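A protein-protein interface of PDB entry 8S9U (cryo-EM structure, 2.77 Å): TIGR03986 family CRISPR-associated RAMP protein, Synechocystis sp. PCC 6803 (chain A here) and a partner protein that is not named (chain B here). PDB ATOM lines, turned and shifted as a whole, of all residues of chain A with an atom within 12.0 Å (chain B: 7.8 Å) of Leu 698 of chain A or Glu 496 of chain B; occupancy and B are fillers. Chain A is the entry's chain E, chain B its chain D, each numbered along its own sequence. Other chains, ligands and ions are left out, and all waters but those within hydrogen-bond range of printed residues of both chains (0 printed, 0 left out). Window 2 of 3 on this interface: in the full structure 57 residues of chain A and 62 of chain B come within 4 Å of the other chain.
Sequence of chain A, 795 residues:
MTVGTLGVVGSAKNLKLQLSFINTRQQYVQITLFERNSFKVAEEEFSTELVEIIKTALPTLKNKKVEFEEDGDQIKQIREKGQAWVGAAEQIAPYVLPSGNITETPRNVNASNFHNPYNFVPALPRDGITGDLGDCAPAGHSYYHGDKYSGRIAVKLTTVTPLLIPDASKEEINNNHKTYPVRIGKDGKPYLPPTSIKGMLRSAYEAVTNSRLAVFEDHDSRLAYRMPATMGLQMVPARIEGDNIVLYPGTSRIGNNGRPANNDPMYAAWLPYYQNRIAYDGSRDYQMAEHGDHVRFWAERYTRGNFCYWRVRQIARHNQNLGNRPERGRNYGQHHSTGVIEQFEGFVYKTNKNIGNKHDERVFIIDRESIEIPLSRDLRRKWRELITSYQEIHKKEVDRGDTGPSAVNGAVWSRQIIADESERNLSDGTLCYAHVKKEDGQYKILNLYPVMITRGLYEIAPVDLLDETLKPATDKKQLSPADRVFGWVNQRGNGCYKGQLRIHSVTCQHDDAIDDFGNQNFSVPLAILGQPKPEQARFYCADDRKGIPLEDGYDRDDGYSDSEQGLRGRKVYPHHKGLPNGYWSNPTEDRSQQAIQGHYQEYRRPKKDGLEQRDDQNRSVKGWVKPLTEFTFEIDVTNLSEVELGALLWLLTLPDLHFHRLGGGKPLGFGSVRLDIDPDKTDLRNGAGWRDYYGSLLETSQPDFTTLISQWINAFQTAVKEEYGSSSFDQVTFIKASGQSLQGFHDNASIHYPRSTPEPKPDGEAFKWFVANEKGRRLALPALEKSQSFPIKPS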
ATOM      1  N   ASP A 683      -2.318  -2.372 -11.205  1.00  0.00           N
ATOM      2  CA  ASP A 683      -2.628  -1.977 -12.576  1.00  0.00           C
ATOM      3  C   ASP A 683      -3.871  -1.090 -12.524  1.00  0.00           C
ATOM      4  O   ASP A 683      -4.998  -1.532 -12.716  1.00  0.00           O
ATOM      5  CB  ASP A 683      -2.848  -3.198 -13.468  1.00  0.00           C
ATOM      6  CG  ASP A 683      -3.194  -2.834 -14.902  1.00  0.00           C
ATOM      7  OD1 ASP A 683      -3.142  -1.643 -15.264  1.00  0.00           O
ATOM      8  OD2 ASP A 683      -3.511  -3.751 -15.682  1.00  0.00           O
ATOM      9  N   ARG A 685      -5.882   2.158 -14.116  1.00  0.00           N
ATOM     10  CA  ARG A 685      -6.041   3.025 -15.273  1.00  0.00           C
ATOM     11  C   ARG A 685      -7.394   3.699 -15.196  1.00  0.00           C
ATOM     12  O   ARG A 685      -8.362   3.113 -14.721  1.00  0.00           O
ATOM     13  CB  ARG A 685      -5.929   2.296 -16.611  1.00  0.00           C
ATOM     14  CG  ARG A 685      -5.101   1.065 -16.601  1.00  0.00           C
ATOM     15  CD  ARG A 685      -5.078   0.449 -17.955  1.00  0.00           C
ATOM     16  NE  ARG A 685      -4.371  -0.817 -17.942  1.00  0.00           N
ATOM     17  CZ  ARG A 685      -3.895  -1.402 -19.027  1.00  0.00           C
ATOM     18  NH1 ARG A 685      -3.953  -0.774 -20.185  1.00  0.00           N
ATOM     19  NH2 ARG A 685      -3.271  -2.560 -18.935  1.00  0.00           N
ATOM     20  N   GLY A 689      -7.684   4.914 -20.254  1.00  0.00           N
ATOM     21  CA  GLY A 689      -6.747   3.816 -20.353  1.00  0.00           C
ATOM     22  C   GLY A 689      -7.367   2.458 -20.557  1.00  0.00           C
ATOM     23  O   GLY A 689      -6.692   1.559 -21.059  1.00  0.00           O
ATOM     24  N   TRP A 690      -8.615   2.267 -20.145  1.00  0.00           N
ATOM     25  CA  TRP A 690      -9.328   1.042 -20.482  1.00  0.00           C
ATOM     26  C   TRP A 690      -9.893   1.039 -21.893  1.00  0.00           C
ATOM     27  O   TRP A 690     -10.011  -0.029 -22.493  1.00  0.00           O
ATOM     28  CB  TRP A 690     -10.425   0.769 -19.464  1.00  0.00           C
ATOM     29  CG  TRP A 690      -9.882   0.526 -18.118  1.00  0.00           C
ATOM     30  CD1 TRP A 690     -10.013   1.317 -17.037  1.00  0.00           C
ATOM     31  CD2 TRP A 690      -9.062  -0.569 -17.717  1.00  0.00           C
ATOM     32  NE1 TRP A 690      -9.354   0.779 -15.973  1.00  0.00           N
ATOM     33  CE2 TRP A 690      -8.756  -0.383 -16.368  1.00  0.00           C
ATOM     34  CE3 TRP A 690      -8.564  -1.698 -18.370  1.00  0.00           C
ATOM     35  CZ2 TRP A 690      -7.978  -1.276 -15.656  1.00  0.00           C
ATOM     36  CZ3 TRP A 690      -7.796  -2.577 -17.662  1.00  0.00           C
ATOM     37  CH2 TRP A 690      -7.508  -2.366 -16.321  1.00  0.00           C
ATOM     38  N   ARG A 691     -10.266   2.193 -22.439  1.00  0.00           N
ATOM     39  CA  ARG A 691     -10.613   2.238 -23.854  1.00  0.00           C
ATOM     40  C   ARG A 691      -9.458   1.803 -24.730  1.00  0.00           C
ATOM     41  O   ARG A 691      -9.675   1.236 -25.803  1.00  0.00           O
ATOM     42  CB  ARG A 691     -11.023   3.642 -24.249  1.00  0.00           C
ATOM     43  CG  ARG A 691     -12.374   4.056 -23.828  1.00  0.00           C
ATOM     44  CD  ARG A 691     -12.773   5.271 -24.614  1.00  0.00           C
ATOM     45  NE  ARG A 691     -12.082   6.459 -24.124  1.00  0.00           N
ATOM     46  CZ  ARG A 691     -11.029   7.011 -24.713  1.00  0.00           C
ATOM     47  NH1 ARG A 691     -10.538   6.489 -25.826  1.00  0.00           N
ATOM     48  NH2 ARG A 691     -10.468   8.088 -24.189  1.00  0.00           N
ATOM     49  N   ASP A 692      -8.232   2.110 -24.324  1.00  0.00           N
ATOM     50  CA  ASP A 692      -7.063   1.627 -25.041  1.00  0.00           C
ATOM     51  C   ASP A 692      -6.861   0.135 -24.835  1.00  0.00           C
ATOM     52  O   ASP A 692      -6.540  -0.589 -25.779  1.00  0.00           O
ATOM     53  CB  ASP A 692      -5.829   2.398 -24.600  1.00  0.00           C
ATOM     54  CG  ASP A 692      -5.920   3.870 -24.928  1.00  0.00           C
ATOM     55  OD1 ASP A 692      -6.763   4.246 -25.766  1.00  0.00           O
ATOM     56  OD2 ASP A 692      -5.142   4.653 -24.350  1.00  0.00           O
ATOM     57  N   TYR A 693      -7.025  -0.338 -23.603  1.00  0.00           N
ATOM     58  CA  TYR A 693      -6.887  -1.760 -23.310  1.00  0.00           C
ATOM     59  C   TYR A 693      -7.895  -2.602 -24.080  1.00  0.00           C
ATOM     60  O   TYR A 693      -7.539  -3.621 -24.674  1.00  0.00           O
ATOM     61  CB  TYR A 693      -7.044  -1.973 -21.811  1.00  0.00           C
ATOM     62  CG  TYR A 693      -6.909  -3.388 -21.340  1.00  0.00           C
ATOM     63  CD1 TYR A 693      -5.673  -3.978 -21.229  1.00  0.00           C
ATOM     64  CD2 TYR A 693      -8.017  -4.125 -20.997  1.00  0.00           C
ATOM     65  CE1 TYR A 693      -5.547  -5.251 -20.783  1.00  0.00           C
ATOM     66  CE2 TYR A 693      -7.899  -5.400 -20.561  1.00  0.00           C
ATOM     67  CZ  TYR A 693      -6.662  -5.960 -20.454  1.00  0.00           C
ATOM     68  OH  TYR A 693      -6.529  -7.249 -20.016  1.00  0.00           O
ATOM     69  N   TYR A 694      -9.156  -2.197 -24.082  1.00  0.00           N
ATOM     70  CA  TYR A 694     -10.175  -2.897 -24.849  1.00  0.00           C
ATOM     71  C   TYR A 694     -10.192  -2.507 -26.309  1.00  0.00           C
ATOM     72  O   TYR A 694     -11.014  -3.028 -27.058  1.00  0.00           O
ATOM     73  CB  TYR A 694     -11.548  -2.654 -24.248  1.00  0.00           C
ATOM     74  CG  TYR A 694     -11.684  -3.195 -22.863  1.00  0.00           C
ATOM     75  CD1 TYR A 694     -11.449  -4.526 -22.600  1.00  0.00           C
ATOM     76  CD2 TYR A 694     -12.048  -2.379 -21.817  1.00  0.00           C
ATOM     77  CE1 TYR A 694     -11.570  -5.022 -21.340  1.00  0.00           C
ATOM     78  CE2 TYR A 694     -12.169  -2.870 -20.558  1.00  0.00           C
ATOM     79  CZ  TYR A 694     -11.933  -4.187 -20.326  1.00  0.00           C
ATOM     80  OH  TYR A 694     -12.061  -4.677 -19.060  1.00  0.00           O
ATOM     81  N   GLY A 695      -9.351  -1.568 -26.722  1.00  0.00           N
ATOM     82  CA  GLY A 695      -9.252  -1.238 -28.125  1.00  0.00           C
ATOM     83  C   GLY A 695      -8.589  -2.296 -28.972  1.00  0.00           C
ATOM     84  O   GLY A 695      -8.709  -2.250 -30.196  1.00  0.00           O
ATOM     85  N   SER A 696      -7.902  -3.252 -28.361  1.00  0.00           N
ATOM     86  CA  SER A 696      -7.158  -4.214 -29.150  1.00  0.00           C
ATOM     87  C   SER A 696      -7.120  -5.547 -28.426  1.00  0.00           C
ATOM     88  O   SER A 696      -7.173  -5.600 -27.200  1.00  0.00           O
ATOM     89  CB  SER A 696      -5.742  -3.708 -29.406  1.00  0.00           C
ATOM     90  OG  SER A 696      -5.093  -4.467 -30.402  1.00  0.00           O
ATOM     91  N   LEU A 697      -7.018  -6.623 -29.200  1.00  0.00           N
ATOM     92  CA  LEU A 697      -6.730  -7.939 -28.652  1.00  0.00           C
ATOM     93  C   LEU A 697      -5.248  -8.196 -28.500  1.00  0.00           C
ATOM     94  O   LEU A 697      -4.870  -9.170 -27.848  1.00  0.00           O
ATOM     95  CB  LEU A 697      -7.349  -9.036 -29.516  1.00  0.00           C
ATOM     96  CG  LEU A 697      -8.862  -9.204 -29.416  1.00  0.00           C
ATOM     97  CD1 LEU A 697      -9.595  -8.184 -30.240  1.00  0.00           C
ATOM     98  CD2 LEU A 697      -9.235 -10.578 -29.845  1.00  0.00           C
ATOM     99  N   LEU A 698      -4.413  -7.363 -29.098  1.00  0.00           N
ATOM    100  CA  LEU A 698      -2.981  -7.416 -28.885  1.00  0.00           C
ATOM    101  C   LEU A 698      -2.638  -6.792 -27.544  1.00  0.00           C
ATOM    102  O   LEU A 698      -3.353  -5.928 -27.041  1.00  0.00           O
ATOM    103  CB  LEU A 698      -2.245  -6.689 -30.003  1.00  0.00           C
ATOM    104  CG  LEU A 698      -2.537  -7.202 -31.404  1.00  0.00           C
ATOM    105  CD1 LEU A 698      -1.796  -6.386 -32.420  1.00  0.00           C
ATOM    106  CD2 LEU A 698      -2.099  -8.632 -31.480  1.00  0.00           C
ATOM    107  N   GLU A 699      -1.536  -7.243 -26.963  1.00  0.00           N
ATOM    108  CA  GLU A 699      -1.053  -6.640 -25.734  1.00  0.00           C
ATOM    109  C   GLU A 699      -0.597  -5.210 -25.983  1.00  0.00           C
ATOM    110  O   GLU A 699      -0.117  -4.863 -27.062  1.00  0.00           O
ATOM    111  CB  GLU A 699       0.075  -7.479 -25.144  1.00  0.00           C
ATOM    112  CG  GLU A 699      -0.440  -8.781 -24.554  1.00  0.00           C
ATOM    113  CD  GLU A 699       0.605  -9.542 -23.774  1.00  0.00           C
ATOM    114  OE1 GLU A 699       0.289 -10.003 -22.658  1.00  0.00           O
ATOM    115  OE2 GLU A 699       1.737  -9.685 -24.279  1.00  0.00           O
ATOM    116  N   THR A 700      -0.741  -4.380 -24.957  1.00  0.00           N
ATOM    117  CA  THR A 700      -0.497  -2.952 -25.075  1.00  0.00           C
ATOM    118  C   THR A 700      -0.008  -2.439 -23.730  1.00  0.00           C
ATOM    119  O   THR A 700      -0.202  -3.079 -22.695  1.00  0.00           O
ATOM    120  CB  THR A 700      -1.760  -2.210 -25.529  1.00  0.00           C
ATOM    121  OG1 THR A 700      -1.436  -0.852 -25.847  1.00  0.00           O
ATOM    122  CG2 THR A 700      -2.814  -2.234 -24.445  1.00  0.00           C
ATOM    123  N   SER A 701       0.650  -1.286 -23.753  1.00  0.00           N
ATOM    124  CA  SER A 701       1.319  -0.805 -22.553  1.00  0.00           C
ATOM    125  C   SER A 701       0.308  -0.384 -21.500  1.00  0.00           C
ATOM    126  O   SER A 701      -0.605   0.395 -21.779  1.00  0.00           O
ATOM    127  CB  SER A 701       2.220   0.375 -22.899  1.00  0.00           C
ATOM    128  OG  SER A 701       1.468   1.402 -23.518  1.00  0.00           O
ATOM    129  N   GLN A 702       0.470  -0.904 -20.290  1.00  0.00           N
ATOM    130  CA  GLN A 702      -0.197  -0.333 -19.134  1.00  0.00           C
ATOM    131  C   GLN A 702       0.505   0.948 -18.689  1.00  0.00           C
ATOM    132  O   GLN A 702       1.730   1.034 -18.744  1.00  0.00           O
ATOM    133  CB  GLN A 702      -0.259  -1.352 -18.001  1.00  0.00           C
ATOM    134  CG  GLN A 702       1.020  -1.616 -17.269  1.00  0.00           C
ATOM    135  CD  GLN A 702       0.778  -2.408 -16.009  1.00  0.00           C
ATOM    136  OE1 GLN A 702       0.385  -3.568 -16.064  1.00  0.00           O
ATOM    137  NE2 GLN A 702       1.004  -1.783 -14.862  1.00  0.00           N
ATOM    138  N   PRO A 703      -0.244   1.957 -18.259  1.00  0.00           N
ATOM    139  CA  PRO A 703       0.380   3.132 -17.646  1.00  0.00           C
ATOM    140  C   PRO A 703       1.047   2.818 -16.317  1.00  0.00           C
ATOM    141  O   PRO A 703       0.708   1.860 -15.621  1.00  0.00           O
ATOM    142  CB  PRO A 703      -0.796   4.095 -17.474  1.00  0.00           C
ATOM    143  CG  PRO A 703      -1.973   3.205 -17.338  1.00  0.00           C
ATOM    144  CD  PRO A 703      -1.712   2.063 -18.272  1.00  0.00           C
ATOM    145  N   LEU B 440     -12.449 -10.588 -25.899  1.00  0.00           N
ATOM    146  CA  LEU B 440     -12.155  -9.612 -24.855  1.00  0.00           C
ATOM    147  C   LEU B 440     -12.841  -9.968 -23.549  1.00  0.00           C
ATOM    148  O   LEU B 440     -12.266  -9.786 -22.476  1.00  0.00           O
ATOM    149  CB  LEU B 440     -12.567  -8.214 -25.305  1.00  0.00           C
ATOM    150  CG  LEU B 440     -11.822  -7.589 -26.475  1.00  0.00           C
ATOM    151  CD1 LEU B 440     -12.524  -6.359 -26.906  1.00  0.00           C
ATOM    152  CD2 LEU B 440     -10.423  -7.256 -26.065  1.00  0.00           C
ATOM    153  N   ARG B 443     -10.788 -12.714 -22.126  1.00  0.00           N
ATOM    154  CA  ARG B 443      -9.570 -12.192 -21.521  1.00  0.00           C
ATOM    155  C   ARG B 443      -9.819 -11.655 -20.120  1.00  0.00           C
ATOM    156  O   ARG B 443      -8.960 -11.774 -19.245  1.00  0.00           O
ATOM    157  CB  ARG B 443      -8.947 -11.134 -22.425  1.00  0.00           C
ATOM    158  CG  ARG B 443      -7.577 -10.710 -21.989  1.00  0.00           C
ATOM    159  CD  ARG B 443      -6.913  -9.822 -22.991  1.00  0.00           C
ATOM    160  NE  ARG B 443      -7.469  -8.482 -22.994  1.00  0.00           N
ATOM    161  CZ  ARG B 443      -7.230  -7.598 -23.948  1.00  0.00           C
ATOM    162  NH1 ARG B 443      -6.457  -7.931 -24.956  1.00  0.00           N
ATOM    163  NH2 ARG B 443      -7.780  -6.406 -23.913  1.00  0.00           N
ATOM    164  N   ASN B 490      -4.107 -13.720 -21.532  1.00  0.00           N
ATOM    165  CA  ASN B 490      -4.125 -12.566 -22.409  1.00  0.00           C
ATOM    166  C   ASN B 490      -4.264 -12.929 -23.878  1.00  0.00           C
ATOM    167  O   ASN B 490      -3.895 -12.124 -24.737  1.00  0.00           O
ATOM    168  CB  ASN B 490      -2.866 -11.743 -22.184  1.00  0.00           C
ATOM    169  CG  ASN B 490      -2.804 -11.172 -20.799  1.00  0.00           C
ATOM    170  OD1 ASN B 490      -3.808 -11.099 -20.106  1.00  0.00           O
ATOM    171  ND2 ASN B 490      -1.616 -10.785 -20.373  1.00  0.00           N
ATOM    172  N   LEU B 491      -4.782 -14.118 -24.182  1.00  0.00           N
ATOM    173  CA  LEU B 491      -5.044 -14.617 -25.530  1.00  0.00           C
ATOM    174  C   LEU B 491      -3.799 -14.841 -26.374  1.00  0.00           C
ATOM    175  O   LEU B 491      -3.928 -15.068 -27.575  1.00  0.00           O
ATOM    176  CB  LEU B 491      -5.998 -13.706 -26.307  1.00  0.00           C
ATOM    177  CG  LEU B 491      -7.236 -13.235 -25.561  1.00  0.00           C
ATOM    178  CD1 LEU B 491      -8.021 -12.258 -26.404  1.00  0.00           C
ATOM    179  CD2 LEU B 491      -8.080 -14.425 -25.187  1.00  0.00           C
ATOM    180  N   THR B 492      -2.602 -14.782 -25.803  1.00  0.00           N
ATOM    181  CA  THR B 492      -1.425 -14.827 -26.660  1.00  0.00           C
ATOM    182  C   THR B 492      -1.159 -16.205 -27.247  1.00  0.00           C
ATOM    183  O   THR B 492      -0.161 -16.369 -27.950  1.00  0.00           O
ATOM    184  CB  THR B 492      -0.195 -14.362 -25.893  1.00  0.00           C
ATOM    185  OG1 THR B 492       0.129 -15.329 -24.890  1.00  0.00           O
ATOM    186  CG2 THR B 492      -0.457 -13.027 -25.235  1.00  0.00           C
ATOM    187  N   ASP B 493      -2.014 -17.189 -26.989  1.00  0.00           N
ATOM    188  CA  ASP B 493      -1.961 -18.461 -27.697  1.00  0.00           C
ATOM    189  C   ASP B 493      -2.653 -18.414 -29.049  1.00  0.00           C
ATOM    190  O   ASP B 493      -2.362 -19.254 -29.904  1.00  0.00           O
ATOM    191  CB  ASP B 493      -2.577 -19.560 -26.841  1.00  0.00           C
ATOM    192  CG  ASP B 493      -1.805 -19.798 -25.565  1.00  0.00           C
ATOM    193  OD1 ASP B 493      -0.581 -20.015 -25.639  1.00  0.00           O
ATOM    194  OD2 ASP B 493      -2.419 -19.771 -24.482  1.00  0.00           O
ATOM    195  N   LEU B 494      -3.558 -17.470 -29.262  1.00  0.00           N
ATOM    196  CA  LEU B 494      -4.081 -17.221 -30.595  1.00  0.00           C
ATOM    197  C   LEU B 494      -3.040 -16.507 -31.441  1.00  0.00           C
ATOM    198  O   LEU B 494      -2.276 -15.681 -30.939  1.00  0.00           O
ATOM    199  CB  LEU B 494      -5.345 -16.382 -30.511  1.00  0.00           C
ATOM    200  CG  LEU B 494      -6.577 -17.067 -29.949  1.00  0.00           C
ATOM    201  CD1 LEU B 494      -7.624 -16.047 -29.649  1.00  0.00           C
ATOM    202  CD2 LEU B 494      -7.104 -18.056 -30.938  1.00  0.00           C
ATOM    203  N   ASP B 495      -2.995 -16.846 -32.728  1.00  0.00           N
ATOM    204  CA  ASP B 495      -1.973 -16.296 -33.609  1.00  0.00           C
ATOM    205  C   ASP B 495      -2.067 -14.781 -33.663  1.00  0.00           C
ATOM    206  O   ASP B 495      -3.155 -14.217 -33.793  1.00  0.00           O
ATOM    207  CB  ASP B 495      -2.114 -16.866 -35.017  1.00  0.00           C
ATOM    208  CG  ASP B 495      -2.069 -18.374 -35.041  1.00  0.00           C
ATOM    209  OD1 ASP B 495      -2.542 -18.999 -34.071  1.00  0.00           O
ATOM    210  OD2 ASP B 495      -1.559 -18.938 -36.031  1.00  0.00           O
ATOM    211  N   GLU B 496      -0.912 -14.122 -33.581  1.00  0.00           N
ATOM    212  CA  GLU B 496      -0.902 -12.664 -33.550  1.00  0.00           C
ATOM    213  C   GLU B 496      -1.504 -12.069 -34.813  1.00  0.00           C
ATOM    214  O   GLU B 496      -2.204 -11.053 -34.753  1.00  0.00           O
ATOM    215  CB  GLU B 496       0.516 -12.144 -33.360  1.00  0.00           C
ATOM    216  CG  GLU B 496       0.555 -10.661 -33.093  1.00  0.00           C
ATOM    217  CD  GLU B 496       1.951 -10.151 -32.857  1.00  0.00           C
ATOM    218  OE1 GLU B 496       2.862 -10.559 -33.604  1.00  0.00           O
ATOM    219  OE2 GLU B 496       2.141  -9.349 -31.922  1.00  0.00           O
ATOM    220  N   ALA B 497      -1.250 -12.688 -35.965  1.00  0.00           N
ATOM    221  CA  ALA B 497      -1.850 -12.209 -37.203  1.00  0.00           C
ATOM    222  C   ALA B 497      -3.363 -12.324 -37.178  1.00  0.00           C
ATOM    223  O   ALA B 497      -4.056 -11.522 -37.810  1.00  0.00           O
ATOM    224  CB  ALA B 497      -1.280 -12.976 -38.389  1.00  0.00           C
ATOM    225  N   PHE B 498      -3.891 -13.320 -36.472  1.00  0.00           N
ATOM    226  CA  PHE B 498      -5.333 -13.425 -36.289  1.00  0.00           C
ATOM    227  C   PHE B 498      -5.850 -12.422 -35.271  1.00  0.00           C
ATOM    228  O   PHE B 498      -6.881 -11.783 -35.498  1.00  0.00           O
ATOM    229  CB  PHE B 498      -5.695 -14.844 -35.866  1.00  0.00           C
ATOM    230  CG  PHE B 498      -7.142 -15.033 -35.564  1.00  0.00           C
ATOM    231  CD1 PHE B 498      -8.083 -14.949 -36.558  1.00  0.00           C
ATOM    232  CD2 PHE B 498      -7.556 -15.323 -34.290  1.00  0.00           C
ATOM    233  CE1 PHE B 498      -9.400 -15.127 -36.283  1.00  0.00           C
ATOM    234  CE2 PHE B 498      -8.873 -15.503 -34.014  1.00  0.00           C
ATOM    235  CZ  PHE B 498      -9.796 -15.406 -35.012  1.00  0.00           C
ATOM    236  N   ARG B 499      -5.157 -12.278 -34.142  1.00  0.00           N
ATOM    237  CA  ARG B 499      -5.532 -11.255 -33.176  1.00  0.00           C
ATOM    238  C   ARG B 499      -5.397  -9.850 -33.733  1.00  0.00           C
ATOM    239  O   ARG B 499      -6.121  -8.948 -33.304  1.00  0.00           O
ATOM    240  CB  ARG B 499      -4.704 -11.402 -31.910  1.00  0.00           C
ATOM    241  CG  ARG B 499      -5.154 -12.534 -31.046  1.00  0.00           C
ATOM    242  CD  ARG B 499      -4.350 -12.596 -29.789  1.00  0.00           C
ATOM    243  NE  ARG B 499      -2.981 -13.002 -30.038  1.00  0.00           N
ATOM    244  CZ  ARG B 499      -1.926 -12.323 -29.623  1.00  0.00           C
ATOM    245  NH1 ARG B 499      -2.091 -11.180 -28.983  1.00  0.00           N
ATOM    246  NH2 ARG B 499      -0.708 -12.763 -29.884  1.00  0.00           N
ATOM    247  N   GLN B 500      -4.469  -9.626 -34.659  1.00  0.00           N
ATOM    248  CA  GLN B 500      -4.393  -8.321 -35.303  1.00  0.00           C
ATOM    249  C   GLN B 500      -5.507  -8.126 -36.319  1.00  0.00           C
ATOM    250  O   GLN B 500      -6.009  -7.012 -36.489  1.00  0.00           O
ATOM    251  CB  GLN B 500      -3.039  -8.123 -35.959  1.00  0.00           C
ATOM    252  CG  GLN B 500      -2.825  -6.708 -36.411  1.00  0.00           C
ATOM    253  CD  GLN B 500      -1.372  -6.414 -36.660  1.00  0.00           C
ATOM    254  OE1 GLN B 500      -0.493  -7.142 -36.194  1.00  0.00           O
ATOM    255  NE2 GLN B 500      -1.102  -5.339 -37.392  1.00  0.00           N
ATOM    256  N   ASP B 501      -5.878  -9.181 -37.035  1.00  0.00           N
ATOM    257  CA  ASP B 501      -7.005  -9.084 -37.954  1.00  0.00           C
ATOM    258  C   ASP B 501      -8.301  -8.785 -37.216  1.00  0.00           C
ATOM    259  O   ASP B 501      -9.092  -7.944 -37.647  1.00  0.00           O
ATOM    260  CB  ASP B 501      -7.132 -10.375 -38.753  1.00  0.00           C
ATOM    261  CG  ASP B 501      -8.231 -10.313 -39.780  1.00  0.00           C
ATOM    262  OD1 ASP B 501      -8.420  -9.236 -40.383  1.00  0.00           O
ATOM    263  OD2 ASP B 501      -8.915 -11.336 -39.984  1.00  0.00           O
ATOM    264  N   LEU B 502      -8.559  -9.502 -36.124  1.00  0.00           N
ATOM    265  CA  LEU B 502      -9.694  -9.185 -35.264  1.00  0.00           C
ATOM    266  C   LEU B 502      -9.604  -7.775 -34.706  1.00  0.00           C
ATOM    267  O   LEU B 502     -10.591  -7.035 -34.706  1.00  0.00           O
ATOM    268  CB  LEU B 502      -9.781 -10.194 -34.127  1.00  0.00           C
ATOM    269  CG  LEU B 502     -10.307 -11.566 -34.499  1.00  0.00           C
ATOM    270  CD1 LEU B 502     -10.516 -12.348 -33.252  1.00  0.00           C
ATOM    271  CD2 LEU B 502     -11.610 -11.410 -35.226  1.00  0.00           C
ATOM    272  N   SER B 503      -8.426  -7.388 -34.218  1.00  0.00           N
ATOM    273  CA  SER B 503      -8.237  -6.035 -33.711  1.00  0.00           C
ATOM    274  C   SER B 503      -8.502  -4.979 -34.770  1.00  0.00           C
ATOM    275  O   SER B 503      -8.998  -3.897 -34.456  1.00  0.00           O
ATOM    276  CB  SER B 503      -6.831  -5.883 -33.160  1.00  0.00           C
ATOM    277  OG  SER B 503      -6.626  -6.801 -32.117  1.00  0.00           O
ATOM    278  N   THR B 504      -8.165  -5.257 -36.023  1.00  0.00           N
ATOM    279  CA  THR B 504      -8.433  -4.284 -37.074  1.00  0.00           C
ATOM    280  C   THR B 504      -9.927  -4.119 -37.310  1.00  0.00           C
ATOM    281  O   THR B 504     -10.428  -2.996 -37.409  1.00  0.00           O
ATOM    282  CB  THR B 504      -7.724  -4.685 -38.358  1.00  0.00           C
ATOM    283  OG1 THR B 504      -6.332  -4.855 -38.092  1.00  0.00           O
ATOM    284  CG2 THR B 504      -7.892  -3.622 -39.399  1.00  0.00           C
ATOM    285  N   LYS B 507     -11.371  -2.370 -34.199  1.00  0.00           N
ATOM    286  CA  LYS B 507     -11.131  -0.935 -34.290  1.00  0.00           C
ATOM    287  C   LYS B 507     -11.969  -0.250 -35.363  1.00  0.00           C
ATOM    288  O   LYS B 507     -12.425   0.879 -35.163  1.00  0.00           O
ATOM    289  CB  LYS B 507      -9.650  -0.700 -34.531  1.00  0.00           C
ATOM    290  CG  LYS B 507      -8.823  -1.012 -33.315  1.00  0.00           C
ATOM    291  CD  LYS B 507      -7.350  -0.786 -33.543  1.00  0.00           C
ATOM    292  CE  LYS B 507      -6.594  -0.990 -32.255  1.00  0.00           C
ATOM    293  NZ  LYS B 507      -5.191  -0.518 -32.318  1.00  0.00           N
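The side-chain carboxylate (OE1) of Glu 699 of chain A sits at hydrogen-bond distance from the side-chain amide nitrogen (ND2) of Asn 490 of chain B.
The guanidinium group (NH1) of Arg 443 of chain B is in hydrogen-bond range of the backbone carbonyl oxygen (O) of Ser 696 of chain A (3.3 Å).
The guanidinium group (NH2) of Arg 443 of chain B lies within hydrogen-bond range of the backbone carbonyl oxygen (O) of Tyr 693 of chain A, at 2.9 Å.
The backbone NH (N) of Leu 697 of chain A is in hydrogen-bond range of the side-chain hydroxyl (OG) of Ser 503 of chain B (2.9 Å).
The side-chain hydroxyl (OG) of Ser 503 of chain B lies within hydrogen-bond range of the side-chain hydroxyl (OG) of Ser 696 of chain A (3.3 Å).
The backbone carbonyl oxygen (O) of Arg 499 of chain B lies within hydrogen-bond range of the side-chain hydroxyl (OG) of Ser 503 of chain B (2.5 Å).
OG of Ser 696 of chain A is in hydrogen-bond range of N of Leu 698 of chain A (3.2 Å).
O of Leu 491 of chain B sits close to NE of Arg 499 of chain B (3.4 Å).
Among the printed residues, merely in contact across the chains: Tyr 694 of chain A with Leu 440 of chain B, Gly 695 of chain A with Lys 507 of chain B, Ser 696 of chain A with Leu 440 of chain B, Leu 697 of chain A with Arg 443 of chain B, Leu 697 of chain A with Arg 499 of chain B, Leu 698 of chain A with Glu 496 of chain B, Leu 698 of chain A with Arg 499 of chain B, Leu 698 of chain A with Ser 503 of chain B and Glu 699 of chain A with Thr 492 of chain B.
Leu 698 of chain A touches just these residues of chain B: Glu 496, Arg 499 and Ser 503.
Of the printed residues of chain A, Arg 443 of chain B touches Tyr 693, Ser 696 and Leu 697.
Of the printed residues of chain A, Asn 490 of chain B touches Glu 699 (3.1 Å).
Leu 491 of chain B touches none of the printed residues of chain A.
Of chain A, only Leu 697 and Leu 698 come within 4 Å of Arg 499 of chain B.
No residue of chain A comes within 4 Å of Gln 500 of chain B.
Leu 502 of chain B touches none of the printed residues of chain A.
Of chain A, only Ser 696 (3.3 Å), Leu 697 (2.9 Å) and Leu 698 (3.8 Å) come within 4 Å of Ser 503 of chain B.
The nearest residue of chain B that does not touch Leu 698 of chain A is Gln 500 of chain B (4.1 Å).
The nearest residue of chain A that does not touch Glu 496 of chain B is Glu 699 of chain A (6.5 Å).
Printed residues of chain A that touch a printed residue of chain B: Tyr 693, Tyr 694, Gly 695, Ser 696, Leu 697, Leu 698 and Glu 699.
Hydrophobic or aromatic side chains of chain B within 4 Å of the printed part of chain A: Leu 440.
Among the printed residues, 14 pairs touch across the chains.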
